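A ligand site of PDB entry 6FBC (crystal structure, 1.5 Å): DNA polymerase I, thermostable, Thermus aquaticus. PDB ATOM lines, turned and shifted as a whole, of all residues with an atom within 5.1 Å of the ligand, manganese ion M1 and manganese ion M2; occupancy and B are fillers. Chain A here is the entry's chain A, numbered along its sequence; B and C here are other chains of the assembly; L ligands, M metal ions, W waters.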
ATOM      1  N   ARG A 282     -35.562  -0.604  28.364  1.00  0.00           N
ATOM      2  CA  ARG A 282     -34.456  -0.188  29.207  1.00  0.00           C
ATOM      3  C   ARG A 282     -34.514   1.304  29.512  1.00  0.00           C
ATOM      4  O   ARG A 282     -35.075   2.100  28.739  1.00  0.00           O
ATOM      5  CB  ARG A 282     -33.126  -0.500  28.532  1.00  0.00           C
ATOM      6  CG  ARG A 282     -32.645  -1.910  28.727  1.00  0.00           C
ATOM      7  CD  ARG A 282     -31.246  -2.020  28.196  1.00  0.00           C
ATOM      8  NE  ARG A 282     -30.599  -3.257  28.581  1.00  0.00           N
ATOM      9  CZ  ARG A 282     -29.317  -3.506  28.352  1.00  0.00           C
ATOM     10  NH1 ARG A 282     -28.563  -2.608  27.735  1.00  0.00           N
ATOM     11  NH2 ARG A 282     -28.786  -4.654  28.730  1.00  0.00           N
ATOM     12  N   ASP A 319     -26.033  -6.991  41.371  1.00  0.00           N
ATOM     13  CA  ASP A 319     -26.098  -7.261  39.937  1.00  0.00           C
ATOM     14  C   ASP A 319     -26.689  -8.634  39.691  1.00  0.00           C
ATOM     15  O   ASP A 319     -26.219  -9.620  40.268  1.00  0.00           O
ATOM     16  CB  ASP A 319     -24.692  -7.152  39.314  1.00  0.00           C
ATOM     17  CG  ASP A 319     -24.714  -7.341  37.826  1.00  0.00           C
ATOM     18  OD1 ASP A 319     -25.098  -8.437  37.406  1.00  0.00           O
ATOM     19  OD2 ASP A 319     -24.390  -6.372  37.112  1.00  0.00           O
ATOM     20  N   TYR A 320     -27.718  -8.704  38.842  1.00  0.00           N
ATOM     21  CA  TYR A 320     -28.368  -9.986  38.556  1.00  0.00           C
ATOM     22  C   TYR A 320     -27.407 -10.912  37.846  1.00  0.00           C
ATOM     23  O   TYR A 320     -26.750 -10.511  36.875  1.00  0.00           O
ATOM     24  CB  TYR A 320     -29.618  -9.788  37.701  1.00  0.00           C
ATOM     25  CG  TYR A 320     -30.877  -9.323  38.423  1.00  0.00           C
ATOM     26  CD1 TYR A 320     -31.639 -10.196  39.167  1.00  0.00           C
ATOM     27  CD2 TYR A 320     -31.325  -8.013  38.300  1.00  0.00           C
ATOM     28  CE1 TYR A 320     -32.796  -9.776  39.818  1.00  0.00           C
ATOM     29  CE2 TYR A 320     -32.473  -7.581  38.933  1.00  0.00           C
ATOM     30  CZ  TYR A 320     -33.207  -8.463  39.688  1.00  0.00           C
ATOM     31  OH  TYR A 320     -34.359  -8.019  40.310  1.00  0.00           O
ATOM     32  N   SER A 321     -27.349 -12.159  38.295  1.00  0.00           N
ATOM     33  CA  SER A 321     -26.518 -13.167  37.637  1.00  0.00           C
ATOM     34  C   SER A 321     -27.122 -13.608  36.309  1.00  0.00           C
ATOM     35  O   SER A 321     -28.297 -13.994  36.245  1.00  0.00           O
ATOM     36  CB  SER A 321     -26.345 -14.380  38.550  1.00  0.00           C
ATOM     37  OG  SER A 321     -25.694 -15.449  37.884  1.00  0.00           O
ATOM     38  N   GLN A 322     -26.313 -13.570  35.249  1.00  0.00           N
ATOM     39  CA  GLN A 322     -26.651 -14.192  33.960  1.00  0.00           C
ATOM     40  C   GLN A 322     -28.085 -13.865  33.524  1.00  0.00           C
ATOM     41  O   GLN A 322     -28.832 -14.729  33.073  1.00  0.00           O
ATOM     42  CB  GLN A 322     -26.445 -15.710  34.043  1.00  0.00           C
ATOM     43  CG  GLN A 322     -25.046 -16.164  34.416  1.00  0.00           C
ATOM     44  CD  GLN A 322     -24.948 -17.676  34.555  1.00  0.00           C
ATOM     45  OE1 GLN A 322     -24.797 -18.400  33.567  1.00  0.00           O
ATOM     46  NE2 GLN A 322     -25.072 -18.162  35.779  1.00  0.00           N
ATOM     47  N   ILE A 323     -28.456 -12.596  33.643  1.00  0.00           N
ATOM     48  CA  ILE A 323     -29.876 -12.279  33.759  1.00  0.00           C
ATOM     49  C   ILE A 323     -30.634 -12.610  32.485  1.00  0.00           C
ATOM     50  O   ILE A 323     -31.722 -13.198  32.540  1.00  0.00           O
ATOM     51  CB  ILE A 323     -30.085 -10.811  34.186  1.00  0.00           C
ATOM     52  CG1 ILE A 323     -31.576 -10.537  34.433  1.00  0.00           C
ATOM     53  CG2 ILE A 323     -29.568  -9.829  33.139  1.00  0.00           C
ATOM     54  CD1 ILE A 323     -32.213 -11.430  35.482  1.00  0.00           C
ATOM     55  N   GLU A 324     -30.102 -12.264  31.303  1.00  0.00           N
ATOM     56  CA  GLU A 324     -30.876 -12.519  30.102  1.00  0.00           C
ATOM     57  C   GLU A 324     -30.934 -14.010  29.754  1.00  0.00           C
ATOM     58  O   GLU A 324     -31.883 -14.446  29.098  1.00  0.00           O
ATOM     59  CB  GLU A 324     -30.356 -11.677  28.942  1.00  0.00           C
ATOM     60  CG  GLU A 324     -30.972 -10.266  28.964  1.00  0.00           C
ATOM     61  CD  GLU A 324     -30.606  -9.375  27.779  1.00  0.00           C
ATOM     62  OE1 GLU A 324     -30.378  -9.902  26.670  1.00  0.00           O
ATOM     63  OE2 GLU A 324     -30.532  -8.150  28.002  1.00  0.00           O
ATOM     64  N   LEU A 325     -29.963 -14.804  30.223  1.00  0.00           N
ATOM     65  CA  LEU A 325     -30.076 -16.252  30.027  1.00  0.00           C
ATOM     66  C   LEU A 325     -31.130 -16.845  30.942  1.00  0.00           C
ATOM     67  O   LEU A 325     -31.820 -17.804  30.562  1.00  0.00           O
ATOM     68  CB  LEU A 325     -28.725 -16.932  30.241  1.00  0.00           C
ATOM     69  CG  LEU A 325     -27.654 -16.586  29.212  1.00  0.00           C
ATOM     70  CD1 LEU A 325     -26.293 -17.162  29.627  1.00  0.00           C
ATOM     71  CD2 LEU A 325     -28.047 -17.108  27.821  1.00  0.00           C
ATOM     72  N   HIS A 348     -21.439 -18.431  31.518  1.00  0.00           N
ATOM     73  CA  HIS A 348     -20.328 -17.549  31.176  1.00  0.00           C
ATOM     74  C   HIS A 348     -18.991 -18.171  31.591  1.00  0.00           C
ATOM     75  O   HIS A 348     -18.013 -18.102  30.844  1.00  0.00           O
ATOM     76  CB  HIS A 348     -20.487 -16.178  31.842  1.00  0.00           C
ATOM     77  CG  HIS A 348     -21.693 -15.415  31.389  1.00  0.00           C
ATOM     78  ND1 HIS A 348     -22.324 -15.639  30.180  1.00  0.00           N
ATOM     79  CD2 HIS A 348     -22.386 -14.420  31.991  1.00  0.00           C
ATOM     80  CE1 HIS A 348     -23.347 -14.809  30.058  1.00  0.00           C
ATOM     81  NE2 HIS A 348     -23.409 -14.068  31.146  1.00  0.00           N
ATOM     82  N   ARG A 368     -14.223 -14.006  32.013  1.00  0.00           N
ATOM     83  CA  ARG A 368     -15.650 -14.314  32.092  1.00  0.00           C
ATOM     84  C   ARG A 368     -16.476 -13.239  31.383  1.00  0.00           C
ATOM     85  O   ARG A 368     -17.440 -13.561  30.674  1.00  0.00           O
ATOM     86  CB  ARG A 368     -16.071 -14.444  33.554  1.00  0.00           C
ATOM     87  CG  ARG A 368     -17.487 -14.947  33.756  1.00  0.00           C
ATOM     88  CD  ARG A 368     -17.786 -15.294  35.231  1.00  0.00           C
ATOM     89  NE  ARG A 368     -19.200 -15.605  35.391  1.00  0.00           N
ATOM     90  CZ  ARG A 368     -20.167 -14.697  35.358  1.00  0.00           C
ATOM     91  NH1 ARG A 368     -19.880 -13.414  35.194  1.00  0.00           N
ATOM     92  NH2 ARG A 368     -21.435 -15.069  35.495  1.00  0.00           N
ATOM     93  N   LYS A 372     -18.964 -13.748  28.299  1.00  0.00           N
ATOM     94  CA  LYS A 372     -20.316 -13.210  28.281  1.00  0.00           C
ATOM     95  C   LYS A 372     -20.653 -12.639  26.907  1.00  0.00           C
ATOM     96  O   LYS A 372     -21.733 -12.885  26.361  1.00  0.00           O
ATOM     97  CB  LYS A 372     -20.478 -12.156  29.370  1.00  0.00           C
ATOM     98  CG  LYS A 372     -21.801 -11.384  29.332  1.00  0.00           C
ATOM     99  CD  LYS A 372     -21.595  -9.863  29.450  1.00  0.00           C
ATOM    100  CE  LYS A 372     -21.003  -9.251  28.187  1.00  0.00           C
ATOM    101  NZ  LYS A 372     -20.964  -7.753  28.293  1.00  0.00           N
ATOM    102  N   THR A 373     -19.716 -11.888  26.309  1.00  0.00           N
ATOM    103  CA  THR A 373     -19.941 -11.310  24.999  1.00  0.00           C
ATOM    104  C   THR A 373     -20.196 -12.401  23.964  1.00  0.00           C
ATOM    105  O   THR A 373     -21.062 -12.258  23.103  1.00  0.00           O
ATOM    106  CB  THR A 373     -18.736 -10.461  24.585  1.00  0.00           C
ATOM    107  OG1 THR A 373     -18.449  -9.523  25.624  1.00  0.00           O
ATOM    108  CG2 THR A 373     -18.999  -9.721  23.290  1.00  0.00           C
ATOM    109  N   PHE A 376     -23.853 -14.101  24.464  1.00  0.00           N
ATOM    110  CA  PHE A 376     -24.962 -13.301  23.954  1.00  0.00           C
ATOM    111  C   PHE A 376     -24.794 -13.005  22.468  1.00  0.00           C
ATOM    112  O   PHE A 376     -25.780 -12.976  21.727  1.00  0.00           O
ATOM    113  CB  PHE A 376     -25.094 -12.020  24.776  1.00  0.00           C
ATOM    114  CG  PHE A 376     -25.549 -12.279  26.174  1.00  0.00           C
ATOM    115  CD1 PHE A 376     -26.755 -12.937  26.406  1.00  0.00           C
ATOM    116  CD2 PHE A 376     -24.781 -11.924  27.260  1.00  0.00           C
ATOM    117  CE1 PHE A 376     -27.181 -13.207  27.686  1.00  0.00           C
ATOM    118  CE2 PHE A 376     -25.217 -12.204  28.558  1.00  0.00           C
ATOM    119  CZ  PHE A 376     -26.408 -12.842  28.764  1.00  0.00           C
ATOM    120  N   GLY A 377     -23.552 -12.830  22.010  1.00  0.00           N
ATOM    121  CA  GLY A 377     -23.332 -12.668  20.580  1.00  0.00           C
ATOM    122  C   GLY A 377     -23.919 -13.822  19.800  1.00  0.00           C
ATOM    123  O   GLY A 377     -24.676 -13.641  18.855  1.00  0.00           O
ATOM    124  N   TYR A 380     -27.955 -14.022  19.957  1.00  0.00           N
ATOM    125  CA  TYR A 380     -28.705 -13.047  19.175  1.00  0.00           C
ATOM    126  C   TYR A 380     -28.242 -12.957  17.717  1.00  0.00           C
ATOM    127  O   TYR A 380     -28.591 -11.995  17.034  1.00  0.00           O
ATOM    128  CB  TYR A 380     -28.632 -11.680  19.866  1.00  0.00           C
ATOM    129  CG  TYR A 380     -29.296 -11.692  21.241  1.00  0.00           C
ATOM    130  CD1 TYR A 380     -30.640 -12.025  21.372  1.00  0.00           C
ATOM    131  CD2 TYR A 380     -28.585 -11.352  22.379  1.00  0.00           C
ATOM    132  CE1 TYR A 380     -31.258 -12.049  22.614  1.00  0.00           C
ATOM    133  CE2 TYR A 380     -29.206 -11.357  23.642  1.00  0.00           C
ATOM    134  CZ  TYR A 380     -30.543 -11.709  23.743  1.00  0.00           C
ATOM    135  OH  TYR A 380     -31.196 -11.731  24.960  1.00  0.00           O
ATOM    136  N   ASN A 459     -34.593 -10.212  20.114  1.00  0.00           N
ATOM    137  CA  ASN A 459     -33.856  -9.715  21.271  1.00  0.00           C
ATOM    138  C   ASN A 459     -34.778  -9.001  22.253  1.00  0.00           C
ATOM    139  O   ASN A 459     -34.605  -9.098  23.472  1.00  0.00           O
ATOM    140  CB  ASN A 459     -32.735  -8.788  20.817  1.00  0.00           C
ATOM    141  CG  ASN A 459     -32.080  -8.043  21.966  1.00  0.00           C
ATOM    142  OD1 ASN A 459     -32.478  -6.925  22.313  1.00  0.00           O
ATOM    143  ND2 ASN A 459     -31.062  -8.651  22.571  1.00  0.00           N
ATOM    144  N   VAL A 492     -27.666   0.310  36.428  1.00  0.00           N
ATOM    145  CA  VAL A 492     -26.908  -0.001  35.211  1.00  0.00           C
ATOM    146  C   VAL A 492     -27.503  -1.258  34.583  1.00  0.00           C
ATOM    147  O   VAL A 492     -26.852  -2.289  34.456  1.00  0.00           O
ATOM    148  CB  VAL A 492     -25.395  -0.169  35.493  1.00  0.00           C
ATOM    149  CG1 VAL A 492     -24.622  -0.100  34.195  1.00  0.00           C
ATOM    150  CG2 VAL A 492     -24.886   0.918  36.433  1.00  0.00           C
ATOM    151  N   ASP A 494     -29.052  -4.083  34.878  1.00  0.00           N
ATOM    152  CA  ASP A 494     -29.393  -5.188  35.771  1.00  0.00           C
ATOM    153  C   ASP A 494     -28.659  -5.044  37.090  1.00  0.00           C
ATOM    154  O   ASP A 494     -28.459  -6.028  37.800  1.00  0.00           O
ATOM    155  CB  ASP A 494     -29.076  -6.547  35.134  1.00  0.00           C
ATOM    156  CG  ASP A 494     -27.595  -6.892  35.190  1.00  0.00           C
ATOM    157  OD1 ASP A 494     -26.764  -5.951  35.173  1.00  0.00           O
ATOM    158  OD2 ASP A 494     -27.258  -8.095  35.244  1.00  0.00           O
ATOM    159  N   GLU A 495     -28.278  -3.822  37.430  1.00  0.00           N
ATOM    160  CA  GLU A 495     -27.457  -3.541  38.586  1.00  0.00           C
ATOM    161  C   GLU A 495     -27.984  -2.285  39.266  1.00  0.00           C
ATOM    162  O   GLU A 495     -28.440  -1.349  38.583  1.00  0.00           O
ATOM    163  CB  GLU A 495     -25.969  -3.367  38.179  1.00  0.00           C
ATOM    164  CG  GLU A 495     -25.047  -2.797  39.250  1.00  0.00           C
ATOM    165  CD  GLU A 495     -23.666  -2.466  38.714  1.00  0.00           C
ATOM    166  OE1 GLU A 495     -23.394  -2.712  37.518  1.00  0.00           O
ATOM    167  OE2 GLU A 495     -22.856  -1.946  39.513  1.00  0.00           O
ATOM    168  N   LYS A 540     -18.092  -4.216  43.728  1.00  0.00           N
ATOM    169  CA  LYS A 540     -18.461  -5.273  42.790  1.00  0.00           C
ATOM    170  C   LYS A 540     -17.515  -6.483  42.863  1.00  0.00           C
ATOM    171  O   LYS A 540     -17.558  -7.331  41.975  1.00  0.00           O
ATOM    172  CB  LYS A 540     -18.513  -4.739  41.362  1.00  0.00           C
ATOM    173  CG  LYS A 540     -19.711  -3.827  41.091  1.00  0.00           C
ATOM    174  CD  LYS A 540     -20.206  -3.905  39.653  1.00  0.00           C
ATOM    175  CE  LYS A 540     -21.014  -5.178  39.414  1.00  0.00           C
ATOM    176  NZ  LYS A 540     -21.470  -5.298  37.989  1.00  0.00           N
ATOM    177  O   D4B B  12     -24.101  -2.583  30.627  1.00  0.00           O
ATOM    178  C1' D4B B  12     -25.013  -3.303  29.863  1.00  0.00           C
ATOM    179  C10 D4B B  12     -17.441  -4.795  29.084  1.00  0.00           C
ATOM    180  C11 D4B B  12     -16.205  -5.333  29.358  1.00  0.00           C
ATOM    181  C12 D4B B  12     -17.698  -6.371  27.239  1.00  0.00           C
ATOM    182  C13 D4B B  12     -16.458  -6.903  27.536  1.00  0.00           C
ATOM    183  C14 D4B B  12     -15.715  -6.416  28.609  1.00  0.00           C
ATOM    184  C15 D4B B  12     -14.501  -6.981  29.044  1.00  0.00           C
ATOM    185  C16 D4B B  12     -13.516  -7.564  29.305  1.00  0.00           C
ATOM    186  C2  D4B B  12     -24.826  -4.048  27.504  1.00  0.00           C
ATOM    187  C2' D4B B  12     -25.509  -4.539  30.690  1.00  0.00           C
ATOM    188  C3' D4B B  12     -24.635  -4.509  31.928  1.00  0.00           C
ATOM    189  C4  D4B B  12     -22.818  -4.021  28.833  1.00  0.00           C
ATOM    190  C4' D4B B  12     -24.264  -3.015  31.967  1.00  0.00           C
ATOM    191  C5  D4B B  12     -22.032  -4.329  27.692  1.00  0.00           C
ATOM    192  C5' D4B B  12     -22.901  -2.913  32.710  1.00  0.00           C
ATOM    193  C6  D4B B  12     -22.754  -4.440  26.487  1.00  0.00           C
ATOM    194  C7  D4B B  12     -20.678  -4.599  27.789  1.00  0.00           C
ATOM    195  C8  D4B B  12     -19.535  -4.896  27.900  1.00  0.00           C
ATOM    196  C9  D4B B  12     -18.207  -5.332  28.032  1.00  0.00           C
ATOM    197  N1  D4B B  12     -24.074  -4.331  26.383  1.00  0.00           N
ATOM    198  N3  D4B B  12     -24.174  -3.842  28.730  1.00  0.00           N
ATOM    199  N6  D4B B  12     -22.077  -4.622  25.289  1.00  0.00           N
ATOM    200  O1  D4B B  12     -21.949  -3.612  32.019  1.00  0.00           O
ATOM    201  O2  D4B B  12     -26.051  -4.000  27.455  1.00  0.00           O
ATOM    202  OP1 D4B B  12     -20.390  -3.456  33.976  1.00  0.00           O
ATOM    203  O3' D4B B  12     -25.323  -4.897  33.080  1.00  0.00           O
ATOM    204  P   D4B B  12     -20.298  -3.292  32.444  1.00  0.00           P
ATOM    205  OP2 D4B B  12     -19.561  -4.404  31.724  1.00  0.00           O
ATOM    206  P    DC C   4     -22.540 -10.215  13.059  1.00  0.00           P
ATOM    207  OP1  DC C   4     -21.617  -9.099  13.344  1.00  0.00           O
ATOM    208  OP2  DC C   4     -22.012 -11.536  12.686  1.00  0.00           O
ATOM    209  O5'  DC C   4     -23.412 -10.428  14.364  1.00  0.00           O
ATOM    210  C5'  DC C   4     -24.121  -9.357  14.890  1.00  0.00           C
ATOM    211  C4'  DC C   4     -25.165  -9.846  15.857  1.00  0.00           C
ATOM    212  O4'  DC C   4     -24.516 -10.541  16.948  1.00  0.00           O
ATOM    213  C3'  DC C   4     -25.984  -8.757  16.513  1.00  0.00           C
ATOM    214  O3'  DC C   4     -27.061  -8.375  15.691  1.00  0.00           O
ATOM    215  C2'  DC C   4     -26.417  -9.422  17.812  1.00  0.00           C
ATOM    216  C1'  DC C   4     -25.191 -10.248  18.163  1.00  0.00           C
ATOM    217  N1   DC C   4     -24.225  -9.585  19.095  1.00  0.00           N
ATOM    218  C2   DC C   4     -24.609  -9.373  20.417  1.00  0.00           C
ATOM    219  O2   DC C   4     -25.739  -9.692  20.760  1.00  0.00           O
ATOM    220  N3   DC C   4     -23.729  -8.813  21.267  1.00  0.00           N
ATOM    221  C4   DC C   4     -22.515  -8.474  20.861  1.00  0.00           C
ATOM    222  N4   DC C   4     -21.690  -7.919  21.765  1.00  0.00           N
ATOM    223  C5   DC C   4     -22.089  -8.691  19.511  1.00  0.00           C
ATOM    224  C6   DC C   4     -22.972  -9.251  18.671  1.00  0.00           C
ATOM    225  P    DG C   5     -27.369  -6.823  15.463  1.00  0.00           P
ATOM    226  OP1  DG C   5     -28.281  -6.740  14.292  1.00  0.00           O
ATOM    227  OP2  DG C   5     -26.091  -6.070  15.468  1.00  0.00           O
ATOM    228  O5'  DG C   5     -28.131  -6.417  16.823  1.00  0.00           O
ATOM    229  C5'  DG C   5     -29.431  -6.930  17.058  1.00  0.00           C
ATOM    230  C4'  DG C   5     -29.845  -6.727  18.487  1.00  0.00           C
ATOM    231  O4'  DG C   5     -28.877  -7.369  19.349  1.00  0.00           O
ATOM    232  C3'  DG C   5     -29.883  -5.285  18.967  1.00  0.00           C
ATOM    233  O3'  DG C   5     -31.116  -4.630  18.594  1.00  0.00           O
ATOM    234  C2'  DG C   5     -29.737  -5.458  20.473  1.00  0.00           C
ATOM    235  C1'  DG C   5     -28.781  -6.651  20.561  1.00  0.00           C
ATOM    236  N9   DG C   5     -27.393  -6.284  20.780  1.00  0.00           N
ATOM    237  C8   DG C   5     -26.338  -6.358  19.894  1.00  0.00           C
ATOM    238  N7   DG C   5     -25.204  -5.942  20.394  1.00  0.00           N
ATOM    239  C5   DG C   5     -25.538  -5.596  21.711  1.00  0.00           C
ATOM    240  C6   DG C   5     -24.725  -5.109  22.746  1.00  0.00           C
ATOM    241  O6   DG C   5     -23.503  -4.867  22.723  1.00  0.00           O
ATOM    242  N1   DG C   5     -25.468  -4.878  23.921  1.00  0.00           N
ATOM    243  C2   DG C   5     -26.815  -5.116  24.046  1.00  0.00           C
ATOM    244  N2   DG C   5     -27.369  -4.826  25.232  1.00  0.00           N
ATOM    245  N3   DG C   5     -27.582  -5.582  23.083  1.00  0.00           N
ATOM    246  C4   DG C   5     -26.867  -5.791  21.941  1.00  0.00           C
HETATM  247  N1  LIG L   1     -24.605  -8.376  23.915  1.00  0.00           N
HETATM  248  C1  LIG L   1     -25.953  -8.437  24.177  1.00  0.00           C
HETATM  249  N2  LIG L   1     -26.752  -8.765  23.167  1.00  0.00           N
HETATM  250  N3  LIG L   1     -26.476  -8.208  25.383  1.00  0.00           N
HETATM  251  C2  LIG L   1     -25.546  -7.928  26.301  1.00  0.00           C
HETATM  252  C3  LIG L   1     -24.183  -7.834  26.143  1.00  0.00           C
HETATM  253  C4  LIG L   1     -23.630  -8.087  24.840  1.00  0.00           C
HETATM  254  O1  LIG L   1     -22.441  -8.097  24.534  1.00  0.00           O
HETATM  255  N4  LIG L   1     -23.570  -7.545  27.359  1.00  0.00           N
HETATM  256  C5  LIG L   1     -24.566  -7.500  28.212  1.00  0.00           C
HETATM  257  N5  LIG L   1     -25.781  -7.744  27.647  1.00  0.00           N
HETATM  258  P1  LIG L   1     -24.027  -8.183  32.629  1.00  0.00           P
HETATM  259  P2  LIG L   1     -24.771 -11.045  32.984  1.00  0.00           P
HETATM  260  P3  LIG L   1     -23.183 -11.730  35.272  1.00  0.00           P
HETATM  261  C6  LIG L   1     -27.083  -7.944  28.306  1.00  0.00           C
HETATM  262  O2  LIG L   1     -24.543  -7.881  34.109  1.00  0.00           O
HETATM  263  O3  LIG L   1     -25.970 -10.613  33.694  1.00  0.00           O
HETATM  264  O4  LIG L   1     -23.431 -13.038  35.997  1.00  0.00           O
HETATM  265  C7  LIG L   1     -27.343  -9.418  28.610  1.00  0.00           C
HETATM  266  O5  LIG L   1     -22.771  -7.511  32.364  1.00  0.00           O
HETATM  267  O6  LIG L   1     -25.218 -11.921  31.768  1.00  0.00           O
HETATM  268  O7  LIG L   1     -21.699 -11.437  35.053  1.00  0.00           O
HETATM  269  C8  LIG L   1     -26.848  -9.537  30.048  1.00  0.00           C
HETATM  270  O8  LIG L   1     -27.487 -10.634  30.709  1.00  0.00           O
HETATM  271  N6  LIG L   1     -23.858  -9.790  32.446  1.00  0.00           N
HETATM  272  O9  LIG L   1     -23.774 -11.916  33.802  1.00  0.00           O
HETATM  273  O10 LIG L   1     -23.953 -10.483  35.826  1.00  0.00           O
HETATM  274  C9  LIG L   1     -27.299  -8.199  30.612  1.00  0.00           C
HETATM  275  O11 LIG L   1     -27.062  -7.254  29.552  1.00  0.00           O
HETATM  276  C10 LIG L   1     -26.596  -7.748  31.860  1.00  0.00           C
HETATM  277  O12 LIG L   1     -25.183  -7.763  31.661  1.00  0.00           O
HETATM  278 MN    MN M   1     -24.644  -5.862  35.079  1.00  0.00          MN
HETATM  279 MN    MN M   2     -25.616  -9.277  35.542  1.00  0.00          MN
HETATM  280  O   HOH W   1     -22.333  -5.810  34.499  1.00  0.00           O
HETATM  281  O   HOH W   2     -20.080  -7.507  25.632  1.00  0.00           O
HETATM  282  O   HOH W   3     -20.916 -10.502  32.593  1.00  0.00           O
HETATM  283  O   HOH W   4     -20.725  -6.488  30.758  1.00  0.00           O
HETATM  284  O   HOH W   5     -29.632  -7.828  24.997  1.00  0.00           O
HETATM  285  O   HOH W   6     -21.912  -8.492  35.954  1.00  0.00           O
HETATM  286  O   HOH W   7     -24.294  -3.771  35.690  1.00  0.00           O
HETATM  287  O   HOH W   8     -22.718 -13.286  38.509  1.00  0.00           O
HETATM  288  O   HOH W   9     -23.880 -10.666  38.836  1.00  0.00           O
HETATM  289  O   HOH W  10     -30.302  -6.724  30.225  1.00  0.00           O
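An oxygen (O4) of the ligand sits at hydrogen-bond distance from the backbone NH of Gln 322, 3.0 Å away.
The side-chain amino group of Lys 372 lies within hydrogen-bond range of a nitrogen (N4) of the ligand (2.8 Å).
The guanidinium group of Arg 368 lies within salt-bridge range of an oxygen (O7) of the ligand (2.7 Å).
NE2 of His 348 is in hydrogen-bond range of O6 of the ligand (2.9 Å).
The backbone NH of Glu 324 is in hydrogen-bond range of an oxygen (O8) of the ligand, at 3.1 Å.
A nitrogen (N2) of the ligand is in hydrogen-bond range of O2 of DC 4 of chain C (2.8 Å).
The backbone NH of Ile 323 lies close to an oxygen (O3) of the ligand (3.2 Å).
The guanidinium group (NH2) of Arg 282 sits at hydrogen-bond distance from an oxygen (O11) of the ligand.
A nitrogen (N2) of the ligand sits close to N3 of DG 5 of chain C (3.3 Å).
O2 of D4B 12 of chain B lies close to N2 of DG 5 of chain C.
The side-chain carboxylate (OD2) of Asp 319 lies close to the side-chain amino group (NZ) of Lys 540.
OH of Tyr 380 lies within hydrogen-bond range of OE1 of Glu 324 (2.6 Å).
O2 of D4B 12 of chain B is in hydrogen-bond range of the guanidinium group of Arg 282, 2.9 Å away.
OG of Ser 321 is in hydrogen-bond range of NE2 of Gln 322.
The side-chain carboxylate of Glu 324 lies within salt-bridge range of the guanidinium group of Arg 282, 3.97 Å away.
CA of Ser 321 touches O4 of the ligand (3.5 Å).
CZ of Phe 376 touches O8 of the ligand, at 3.1 Å.
CD2 of Tyr 380 touches N2 of the ligand, 3.3 Å away.
Hydrophobic or aromatic side chains within 4 Å of the ligand: Ile 323, His 348, Phe 376 and Tyr 380.
Along chain A the residues within 4 Å of the ligand span positions 282 to 494.
Of the 23 residues printed, 3 come within 4 Å of manganese ion M1.
Of the 23 residues printed, 3 come within 4 Å of manganese ion M2.
The side-chain carboxylate (OD2) of Asp 319 is bound to manganese ion M1 (2.1 Å).
Manganese ion M1 is bound by OD1 of Asp 494, at 2.1 Å.
Manganese ion M1 is bound by water W7.
An oxygen (O2) of the ligand is bound to manganese ion M1, 2.2 Å away.
O3' of D4B 12 of chain B binds manganese ion M1.
Water W1 is bound to manganese ion M1.
Manganese ion M2 is bound by the side-chain carboxylate (OD2) of Asp 494 (2.0 Å), an oxygen (O10) of the ligand (2.1 Å), the side-chain carboxylate (OD1) of Asp 319 (2.1 Å), the backbone carbonyl oxygen (O) of Tyr 320 (2.1 Å), an oxygen (O2) of the ligand (2.3 Å) and an oxygen (O3) of the ligand (2.3 Å).
Manganese ion M2 has six donor atoms within binding distance.
Water W1 lies within hydrogen-bond range of O5 of the ligand and OP1 of D4B 12 of chain B.
Water W2 lies within hydrogen-bond range of the side-chain hydroxyl (OG1) of Thr 373, an oxygen (O1) of the ligand and the side-chain amino group (NZ) of Lys 372.
Water W4 lies within hydrogen-bond range of OP2 of D4B 12 of chain B (2.6 Å), the side-chain amino group of Lys 372 (2.8 Å) and an oxygen (O5) of the ligand (2.8 Å).
Water W5 lies within hydrogen-bond range of the side-chain carboxylate of Glu 324, the side-chain amide nitrogen of Asn 459 and a nitrogen (N3) of the ligand.
Water W10 lies within hydrogen-bond range of the side-chain carboxylate of Glu 324, the guanidinium group of Arg 282 and an oxygen (O11) of the ligand.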
